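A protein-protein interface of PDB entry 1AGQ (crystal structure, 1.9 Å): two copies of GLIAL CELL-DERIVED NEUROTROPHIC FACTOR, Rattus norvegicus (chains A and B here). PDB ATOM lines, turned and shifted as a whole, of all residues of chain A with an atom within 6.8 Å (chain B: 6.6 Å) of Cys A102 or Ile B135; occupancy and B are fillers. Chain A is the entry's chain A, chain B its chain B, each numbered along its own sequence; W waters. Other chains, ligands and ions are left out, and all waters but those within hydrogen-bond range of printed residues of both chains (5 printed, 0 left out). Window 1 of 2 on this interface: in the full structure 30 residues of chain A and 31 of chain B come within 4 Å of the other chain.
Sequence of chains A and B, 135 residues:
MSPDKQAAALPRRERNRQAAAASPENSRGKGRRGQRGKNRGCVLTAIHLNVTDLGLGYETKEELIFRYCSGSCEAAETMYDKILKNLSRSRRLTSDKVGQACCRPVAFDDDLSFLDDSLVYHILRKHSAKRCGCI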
ATOM      1  N   CYS A  42       5.625 -14.278   4.251  1.00  0.00           N
ATOM      2  CA  CYS A  42       4.419 -14.359   5.078  1.00  0.00           C
ATOM      3  C   CYS A  42       4.059 -12.896   5.327  1.00  0.00           C
ATOM      4  O   CYS A  42       4.751 -12.188   6.055  1.00  0.00           O
ATOM      5  CB  CYS A  42       4.712 -15.062   6.409  1.00  0.00           C
ATOM      6  SG  CYS A  42       3.358 -14.931   7.627  1.00  0.00           S
ATOM      7  N   GLY A  71       1.275 -16.285   2.652  1.00  0.00           N
ATOM      8  CA  GLY A  71       2.663 -16.268   2.233  1.00  0.00           C
ATOM      9  C   GLY A  71       3.394 -17.506   2.722  1.00  0.00           C
ATOM     10  O   GLY A  71       2.943 -18.224   3.619  1.00  0.00           O
ATOM     11  N   SER A  72       4.560 -17.736   2.143  1.00  0.00           N
ATOM     12  CA  SER A  72       5.359 -18.904   2.469  1.00  0.00           C
ATOM     13  C   SER A  72       6.137 -18.833   3.767  1.00  0.00           C
ATOM     14  O   SER A  72       6.555 -17.763   4.205  1.00  0.00           O
ATOM     15  CB  SER A  72       6.325 -19.178   1.317  1.00  0.00           C
ATOM     16  N   CYS A  73       6.338 -20.005   4.367  1.00  0.00           N
ATOM     17  CA  CYS A  73       7.102 -20.137   5.600  1.00  0.00           C
ATOM     18  C   CYS A  73       8.149 -21.217   5.366  1.00  0.00           C
ATOM     19  O   CYS A  73       8.338 -22.116   6.187  1.00  0.00           O
ATOM     20  CB  CYS A  73       6.186 -20.541   6.744  1.00  0.00           C
ATOM     21  SG  CYS A  73       5.194 -19.135   7.293  1.00  0.00           S
ATOM     22  N   GLY A  99       3.622 -31.620   9.386  1.00  0.00           N
ATOM     23  CA  GLY A  99       3.760 -30.607  10.414  1.00  0.00           C
ATOM     24  C   GLY A  99       4.481 -29.307  10.103  1.00  0.00           C
ATOM     25  O   GLY A  99       4.922 -28.631  11.031  1.00  0.00           O
ATOM     26  N   GLN A 100       4.580 -28.923   8.826  1.00  0.00           N
ATOM     27  CA  GLN A 100       5.276 -27.681   8.441  1.00  0.00           C
ATOM     28  C   GLN A 100       4.649 -26.419   9.044  1.00  0.00           C
ATOM     29  O   GLN A 100       3.443 -26.382   9.313  1.00  0.00           O
ATOM     30  CB  GLN A 100       5.303 -27.541   6.917  1.00  0.00           C
ATOM     31  CG  GLN A 100       3.925 -27.286   6.333  1.00  0.00           C
ATOM     32  CD  GLN A 100       3.934 -27.051   4.837  1.00  0.00           C
ATOM     33  OE1 GLN A 100       2.895 -27.157   4.179  1.00  0.00           O
ATOM     34  NE2 GLN A 100       5.104 -26.727   4.288  1.00  0.00           N
ATOM     35  N   ALA A 101       5.469 -25.389   9.243  1.00  0.00           N
ATOM     36  CA  ALA A 101       5.021 -24.124   9.820  1.00  0.00           C
ATOM     37  C   ALA A 101       4.116 -23.393   8.837  1.00  0.00           C
ATOM     38  O   ALA A 101       4.199 -23.616   7.626  1.00  0.00           O
ATOM     39  CB  ALA A 101       6.215 -23.247  10.159  1.00  0.00           C
ATOM     40  N   CYS A 102       3.261 -22.516   9.360  1.00  0.00           N
ATOM     41  CA  CYS A 102       2.339 -21.772   8.502  1.00  0.00           C
ATOM     42  C   CYS A 102       2.268 -20.297   8.854  1.00  0.00           C
ATOM     43  O   CYS A 102       2.524 -19.885   9.998  1.00  0.00           O
ATOM     44  CB  CYS A 102       0.925 -22.394   8.553  1.00  0.00           C
ATOM     45  SG  CYS A 102       0.133 -22.500  10.197  1.00  0.00           S
ATOM     46  N   CYS A 103       1.948 -19.501   7.836  1.00  0.00           N
ATOM     47  CA  CYS A 103       1.830 -18.055   7.973  1.00  0.00           C
ATOM     48  C   CYS A 103       0.458 -17.800   8.616  1.00  0.00           C
ATOM     49  O   CYS A 103      -0.584 -18.046   7.995  1.00  0.00           O
ATOM     50  CB  CYS A 103       1.906 -17.409   6.584  1.00  0.00           C
ATOM     51  SG  CYS A 103       1.731 -15.602   6.639  1.00  0.00           S
ATOM     52  N   ARG A 104       0.475 -17.307   9.851  1.00  0.00           N
ATOM     53  CA  ARG A 104      -0.740 -17.085  10.637  1.00  0.00           C
ATOM     54  C   ARG A 104      -0.667 -15.840  11.501  1.00  0.00           C
ATOM     55  O   ARG A 104       0.398 -15.257  11.675  1.00  0.00           O
ATOM     56  CB  ARG A 104      -0.936 -18.298  11.573  1.00  0.00           C
ATOM     57  CG  ARG A 104      -1.042 -19.610  10.850  1.00  0.00           C
ATOM     58  CD  ARG A 104      -2.464 -19.832  10.350  1.00  0.00           C
ATOM     59  NE  ARG A 104      -3.390 -19.822  11.470  1.00  0.00           N
ATOM     60  CZ  ARG A 104      -4.702 -19.685  11.363  1.00  0.00           C
ATOM     61  NH1 ARG A 104      -5.266 -19.546  10.169  1.00  0.00           N
ATOM     62  NH2 ARG A 104      -5.435 -19.667  12.464  1.00  0.00           N
ATOM     63  N   PRO A 105      -1.823 -15.394  12.044  1.00  0.00           N
ATOM     64  CA  PRO A 105      -1.810 -14.212  12.909  1.00  0.00           C
ATOM     65  C   PRO A 105      -1.051 -14.521  14.208  1.00  0.00           C
ATOM     66  O   PRO A 105      -1.225 -15.594  14.781  1.00  0.00           O
ATOM     67  CB  PRO A 105      -3.301 -13.950  13.209  1.00  0.00           C
ATOM     68  CG  PRO A 105      -4.047 -14.733  12.202  1.00  0.00           C
ATOM     69  CD  PRO A 105      -3.181 -15.904  11.822  1.00  0.00           C
ATOM     70  N   GLY A 133       3.023 -13.978  11.256  1.00  0.00           N
ATOM     71  CA  GLY A 133       4.290 -14.649  11.504  1.00  0.00           C
ATOM     72  C   GLY A 133       4.215 -16.125  11.168  1.00  0.00           C
ATOM     73  O   GLY A 133       3.123 -16.669  11.049  1.00  0.00           O
ATOM     74  N   CYS A 134       5.367 -16.777  10.999  1.00  0.00           N
ATOM     75  CA  CYS A 134       5.377 -18.205  10.686  1.00  0.00           C
ATOM     76  C   CYS A 134       5.371 -18.954  12.015  1.00  0.00           C
ATOM     77  O   CYS A 134       6.271 -18.769  12.839  1.00  0.00           O
ATOM     78  CB  CYS A 134       6.630 -18.562   9.889  1.00  0.00           C
ATOM     79  SG  CYS A 134       6.539 -17.917   8.192  1.00  0.00           S
ATOM     80  N   ILE A 135       4.356 -19.782  12.235  1.00  0.00           N
ATOM     81  CA  ILE A 135       4.255 -20.512  13.498  1.00  0.00           C
ATOM     82  C   ILE A 135       3.892 -21.984  13.340  1.00  0.00           C
ATOM     83  O   ILE A 135       3.557 -22.386  12.210  1.00  0.00           O
ATOM     84  CB  ILE A 135       3.221 -19.853  14.423  1.00  0.00           C
ATOM     85  CG1 ILE A 135       1.827 -19.916  13.785  1.00  0.00           C
ATOM     86  CG2 ILE A 135       3.618 -18.420  14.691  1.00  0.00           C
ATOM     87  CD1 ILE A 135       0.713 -19.330  14.667  1.00  0.00           C
ATOM     88  OXT ILE A 135       3.946 -22.714  14.357  1.00  0.00           O
ATOM     89  N   CYS B  73      -6.584 -29.898  10.372  1.00  0.00           N
ATOM     90  CA  CYS B  73      -7.110 -28.777  11.156  1.00  0.00           C
ATOM     91  C   CYS B  73      -8.252 -28.140  10.383  1.00  0.00           C
ATOM     92  O   CYS B  73      -8.391 -26.916  10.351  1.00  0.00           O
ATOM     93  CB  CYS B  73      -6.034 -27.729  11.380  1.00  0.00           C
ATOM     94  SG  CYS B  73      -4.844 -28.258  12.633  1.00  0.00           S
ATOM     95  N   GLU B  77     -11.373 -22.948  14.654  1.00  0.00           N
ATOM     96  CA  GLU B  77     -11.370 -22.887  16.111  1.00  0.00           C
ATOM     97  C   GLU B  77     -11.338 -21.460  16.601  1.00  0.00           C
ATOM     98  O   GLU B  77     -11.343 -21.203  17.807  1.00  0.00           O
ATOM     99  CB  GLU B  77     -10.156 -23.630  16.671  1.00  0.00           C
ATOM    100  CG  GLU B  77     -10.298 -25.128  16.660  1.00  0.00           C
ATOM    101  CD  GLU B  77      -9.187 -25.812  17.428  1.00  0.00           C
ATOM    102  OE1 GLU B  77      -8.718 -25.217  18.429  1.00  0.00           O
ATOM    103  OE2 GLU B  77      -8.787 -26.923  17.030  1.00  0.00           O
ATOM    104  N   THR B  78     -11.290 -20.525  15.659  1.00  0.00           N
ATOM    105  CA  THR B  78     -11.244 -19.117  16.008  1.00  0.00           C
ATOM    106  C   THR B  78     -12.202 -18.342  15.116  1.00  0.00           C
ATOM    107  O   THR B  78     -12.639 -18.839  14.067  1.00  0.00           O
ATOM    108  CB  THR B  78      -9.816 -18.565  15.816  1.00  0.00           C
ATOM    109  OG1 THR B  78      -9.532 -18.454  14.413  1.00  0.00           O
ATOM    110  CG2 THR B  78      -8.781 -19.505  16.456  1.00  0.00           C
ATOM    111  N   ASP B  81     -10.579 -17.890  11.671  1.00  0.00           N
ATOM    112  CA  ASP B  81     -10.676 -19.003  10.748  1.00  0.00           C
ATOM    113  C   ASP B  81     -12.073 -19.203  10.184  1.00  0.00           C
ATOM    114  O   ASP B  81     -12.232 -19.653   9.061  1.00  0.00           O
ATOM    115  CB  ASP B  81     -10.180 -20.268  11.436  1.00  0.00           C
ATOM    116  CG  ASP B  81      -8.672 -20.278  11.555  1.00  0.00           C
ATOM    117  OD1 ASP B  81      -8.016 -20.071  10.512  1.00  0.00           O
ATOM    118  OD2 ASP B  81      -8.151 -20.469  12.668  1.00  0.00           O
ATOM    119  N   GLY B  99      -3.418 -18.250   4.683  1.00  0.00           N
ATOM    120  CA  GLY B  99      -2.904 -19.377   5.433  1.00  0.00           C
ATOM    121  C   GLY B  99      -3.944 -19.966   6.368  1.00  0.00           C
ATOM    122  O   GLY B  99      -4.427 -19.283   7.273  1.00  0.00           O
ATOM    123  N   GLN B 100      -4.296 -21.229   6.136  1.00  0.00           N
ATOM    124  CA  GLN B 100      -5.263 -21.933   6.981  1.00  0.00           C
ATOM    125  C   GLN B 100      -4.535 -22.390   8.239  1.00  0.00           C
ATOM    126  O   GLN B 100      -3.304 -22.384   8.279  1.00  0.00           O
ATOM    127  CB  GLN B 100      -5.830 -23.156   6.258  1.00  0.00           C
ATOM    128  CG  GLN B 100      -6.814 -22.808   5.164  1.00  0.00           C
ATOM    129  CD  GLN B 100      -6.126 -22.153   3.992  1.00  0.00           C
ATOM    130  OE1 GLN B 100      -4.905 -22.264   3.839  1.00  0.00           O
ATOM    131  NE2 GLN B 100      -6.896 -21.462   3.155  1.00  0.00           N
ATOM    132  N   ALA B 101      -5.289 -22.772   9.267  1.00  0.00           N
ATOM    133  CA  ALA B 101      -4.689 -23.230  10.520  1.00  0.00           C
ATOM    134  C   ALA B 101      -3.908 -24.517  10.280  1.00  0.00           C
ATOM    135  O   ALA B 101      -4.264 -25.323   9.408  1.00  0.00           O
ATOM    136  CB  ALA B 101      -5.782 -23.458  11.571  1.00  0.00           C
ATOM    137  N   CYS B 102      -2.816 -24.700  11.023  1.00  0.00           N
ATOM    138  CA  CYS B 102      -2.012 -25.910  10.862  1.00  0.00           C
ATOM    139  C   CYS B 102      -1.759 -26.595  12.205  1.00  0.00           C
ATOM    140  O   CYS B 102      -1.751 -25.954  13.266  1.00  0.00           O
ATOM    141  CB  CYS B 102      -0.651 -25.611  10.193  1.00  0.00           C
ATOM    142  SG  CYS B 102       0.385 -24.336  10.939  1.00  0.00           S
ATOM    143  N   CYS B 103      -1.549 -27.901  12.141  1.00  0.00           N
ATOM    144  CA  CYS B 103      -1.278 -28.709  13.328  1.00  0.00           C
ATOM    145  C   CYS B 103       0.195 -28.498  13.683  1.00  0.00           C
ATOM    146  O   CYS B 103       1.077 -28.920  12.944  1.00  0.00           O
ATOM    147  CB  CYS B 103      -1.581 -30.176  13.017  1.00  0.00           C
ATOM    148  SG  CYS B 103      -1.358 -31.270  14.451  1.00  0.00           S
ATOM    149  N   ARG B 104       0.438 -27.837  14.806  1.00  0.00           N
ATOM    150  CA  ARG B 104       1.776 -27.469  15.272  1.00  0.00           C
ATOM    151  C   ARG B 104       1.906 -27.566  16.783  1.00  0.00           C
ATOM    152  O   ARG B 104       0.921 -27.736  17.504  1.00  0.00           O
ATOM    153  CB  ARG B 104       2.054 -26.017  14.857  1.00  0.00           C
ATOM    154  CG  ARG B 104       1.916 -25.769  13.373  1.00  0.00           C
ATOM    155  CD  ARG B 104       3.243 -26.033  12.687  1.00  0.00           C
ATOM    156  NE  ARG B 104       4.277 -25.208  13.295  1.00  0.00           N
ATOM    157  CZ  ARG B 104       5.575 -25.395  13.102  1.00  0.00           C
ATOM    158  NH1 ARG B 104       6.015 -26.358  12.341  1.00  0.00           N
ATOM    159  NH2 ARG B 104       6.438 -24.550  13.710  1.00  0.00           N
ATOM    160  N   PRO B 105       3.154 -27.484  17.303  1.00  0.00           N
ATOM    161  CA  PRO B 105       3.267 -27.559  18.759  1.00  0.00           C
ATOM    162  C   PRO B 105       2.713 -26.293  19.394  1.00  0.00           C
ATOM    163  O   PRO B 105       2.977 -25.184  18.918  1.00  0.00           O
ATOM    164  CB  PRO B 105       4.782 -27.671  19.005  1.00  0.00           C
ATOM    165  CG  PRO B 105       5.369 -28.028  17.652  1.00  0.00           C
ATOM    166  CD  PRO B 105       4.456 -27.389  16.646  1.00  0.00           C
ATOM    167  N   VAL B 106       1.931 -26.464  20.456  1.00  0.00           N
ATOM    168  CA  VAL B 106       1.376 -25.336  21.191  1.00  0.00           C
ATOM    169  C   VAL B 106       2.204 -25.234  22.465  1.00  0.00           C
ATOM    170  O   VAL B 106       2.172 -24.238  23.191  1.00  0.00           O
ATOM    171  CB  VAL B 106      -0.135 -25.557  21.498  1.00  0.00           C
ATOM    172  CG1 VAL B 106      -0.921 -25.463  20.205  1.00  0.00           C
ATOM    173  CG2 VAL B 106      -0.375 -26.920  22.115  1.00  0.00           C
ATOM    174  N   GLY B 133      -1.564 -28.527  18.585  1.00  0.00           N
ATOM    175  CA  GLY B 133      -2.806 -27.774  18.463  1.00  0.00           C
ATOM    176  C   GLY B 133      -2.929 -27.132  17.100  1.00  0.00           C
ATOM    177  O   GLY B 133      -1.935 -26.941  16.393  1.00  0.00           O
ATOM    178  N   CYS B 134      -4.158 -26.843  16.692  1.00  0.00           N
ATOM    179  CA  CYS B 134      -4.381 -26.184  15.416  1.00  0.00           C
ATOM    180  C   CYS B 134      -4.203 -24.698  15.677  1.00  0.00           C
ATOM    181  O   CYS B 134      -4.921 -24.114  16.484  1.00  0.00           O
ATOM    182  CB  CYS B 134      -5.788 -26.505  14.906  1.00  0.00           C
ATOM    183  SG  CYS B 134      -5.897 -28.241  14.361  1.00  0.00           S
ATOM    184  N   ILE B 135      -3.221 -24.090  15.020  1.00  0.00           N
ATOM    185  CA  ILE B 135      -2.952 -22.671  15.225  1.00  0.00           C
ATOM    186  C   ILE B 135      -2.780 -21.904  13.920  1.00  0.00           C
ATOM    187  O   ILE B 135      -2.598 -22.556  12.872  1.00  0.00           O
ATOM    188  CB  ILE B 135      -1.683 -22.449  16.099  1.00  0.00           C
ATOM    189  CG1 ILE B 135      -0.453 -23.045  15.415  1.00  0.00           C
ATOM    190  CG2 ILE B 135      -1.885 -23.068  17.473  1.00  0.00           C
ATOM    191  CD1 ILE B 135       0.849 -22.835  16.182  1.00  0.00           C
ATOM    192  OXT ILE B 135      -2.829 -20.652  13.983  1.00  0.00           O
HETATM  193  O   HOH W   1      -3.832 -16.914   7.751  1.00  0.00           O
HETATM  194  O   HOH W   2      -5.379 -19.960  15.887  1.00  0.00           O
HETATM  195  O   HOH W   3       1.408 -28.272  10.135  1.00  0.00           O
HETATM  196  O   HOH W   4       4.663 -23.007  16.792  1.00  0.00           O
HETATM  197  O   HOH W   5       4.382 -29.589  13.529  1.00  0.00           O
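The backbone carbonyl oxygen of Arg A104 lies within hydrogen-bond range of the backbone NH of Gly A133 (2.9 Å). The backbone NH (N) of Cys B102 is in hydrogen-bond range of the chain-end carboxylate (O) of Ile B135. SG of Cys A103 forms a disulfide with SG of Cys A42 (2.0 Å). The backbone NH of Cys A102 is in hydrogen-bond range of the chain-end carboxylate of Ile A135 (2.9 Å). The backbone carbonyl oxygen of Arg B104 sits at hydrogen-bond distance from the backbone NH of Gly B133, 2.8 Å away. SG of Cys A73 forms a disulfide with SG of Cys A134, at 2.0 Å.
Among the printed residues, pairs that only touch across the chains: Arg A104 with Gln B100 (3.4 Å), Gln A100 with Arg B104 (3.4 Å), Ile A135 with Ile B135 (3.6 Å), Cys A103 with Gly B99 (3.7 Å), Cys A102 with Ile B135 (3.8 Å), Ile A135 with Cys B102 (3.9 Å) and Cys A102 with Gln B100 (3.9 Å).
NH1 of Arg A104 is in hydrogen-bond range of O of Gly B99, 3.0 Å away. OXT of Ile A135 is in salt-bridge range of NE of Arg B104 (2.7 Å). N of Ala B101 lies close to NH1 of Arg A104, 3.3 Å away. The guanidinium group of Arg A104 is in salt-bridge range of the side-chain carboxylate of Asp B81, at 2.8 Å. NH1 of Arg B104 sits close to N of Ala A101, at 3.3 Å. The guanidinium group (NE) of Arg A104 lies within salt-bridge range of the chain-end carboxylate (OXT) of Ile B135 (2.7 Å). NH1 of Arg B104 lies within hydrogen-bond range of O of Gly A99. SG of Cys A102 is disulfide-bonded to SG of Cys B102.
Water W1 bridges O of Gly B99 and O of Cys A103. Water W4 bridges OXT of Ile A135 and O of Pro B105. Water W5 bridges O of Gly A99 and O of Cys B103. Water W3 lies within hydrogen-bond range of O of Gln A100 (2.9 Å) and O of Cys B103 (2.9 Å). Water W2 bridges the chain-end carboxylate (OXT) of Ile B135 and the guanidinium group (NH2) of Arg A104.
Gln A100 touches Arg B104, and with the chains exchanged Arg A104 touches Gln B100. Ala A101 touches Arg B104, and with the chains exchanged Arg A104 touches Ala B101. Cys A102 touches its own counterpart, Cys B102. Arg A104 touches Ile B135, and with the chains exchanged Ile A135 touches Arg B104. 11 positions are printed for both chains. Of the 15 pairs that touch across the chains among the printed residues, 12 have their exchanged pair printed and touching as well.
Printed residues of chain B within 4 Å of Gln A100: Arg B104 (3.4 Å). Printed residues of chain B within 4 Å of Cys A103: Gly B99 (3.7 Å). Printed residues of chain A within 4 Å of Asp B81: Arg A104. Printed residues of chain A within 4 Å of Cys B102: Cys A102 (2.0 Å) and Ile A135 (3.9 Å). Cys B103 touches none of the printed residues of chain A. Of the printed residues of chain A, Arg B104 touches Gly A99, Gln A100, Ala A101 and Ile A135. The nearest printed residue of chain B that does not touch Cys A102 is Ala B101 (4.5 Å). The nearest printed residue of chain B that does not touch Ile A135 is Pro B105 (5.2 Å).
Of the 15 printed residues of chain B, 7 touch a printed residue of chain A. Of the 14 printed residues of chain A, 7 touch a printed residue of chain B. Hydrophobic or aromatic side chains of chain A that line the printed part of chain B: Ala A101 and Ile A135. Among the printed residues, Asp or Glu carboxylates within 4 Å of a Lys or Arg side-chain nitrogen of the other chain: Arg A104 with Asp B81 (2.8 Å).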
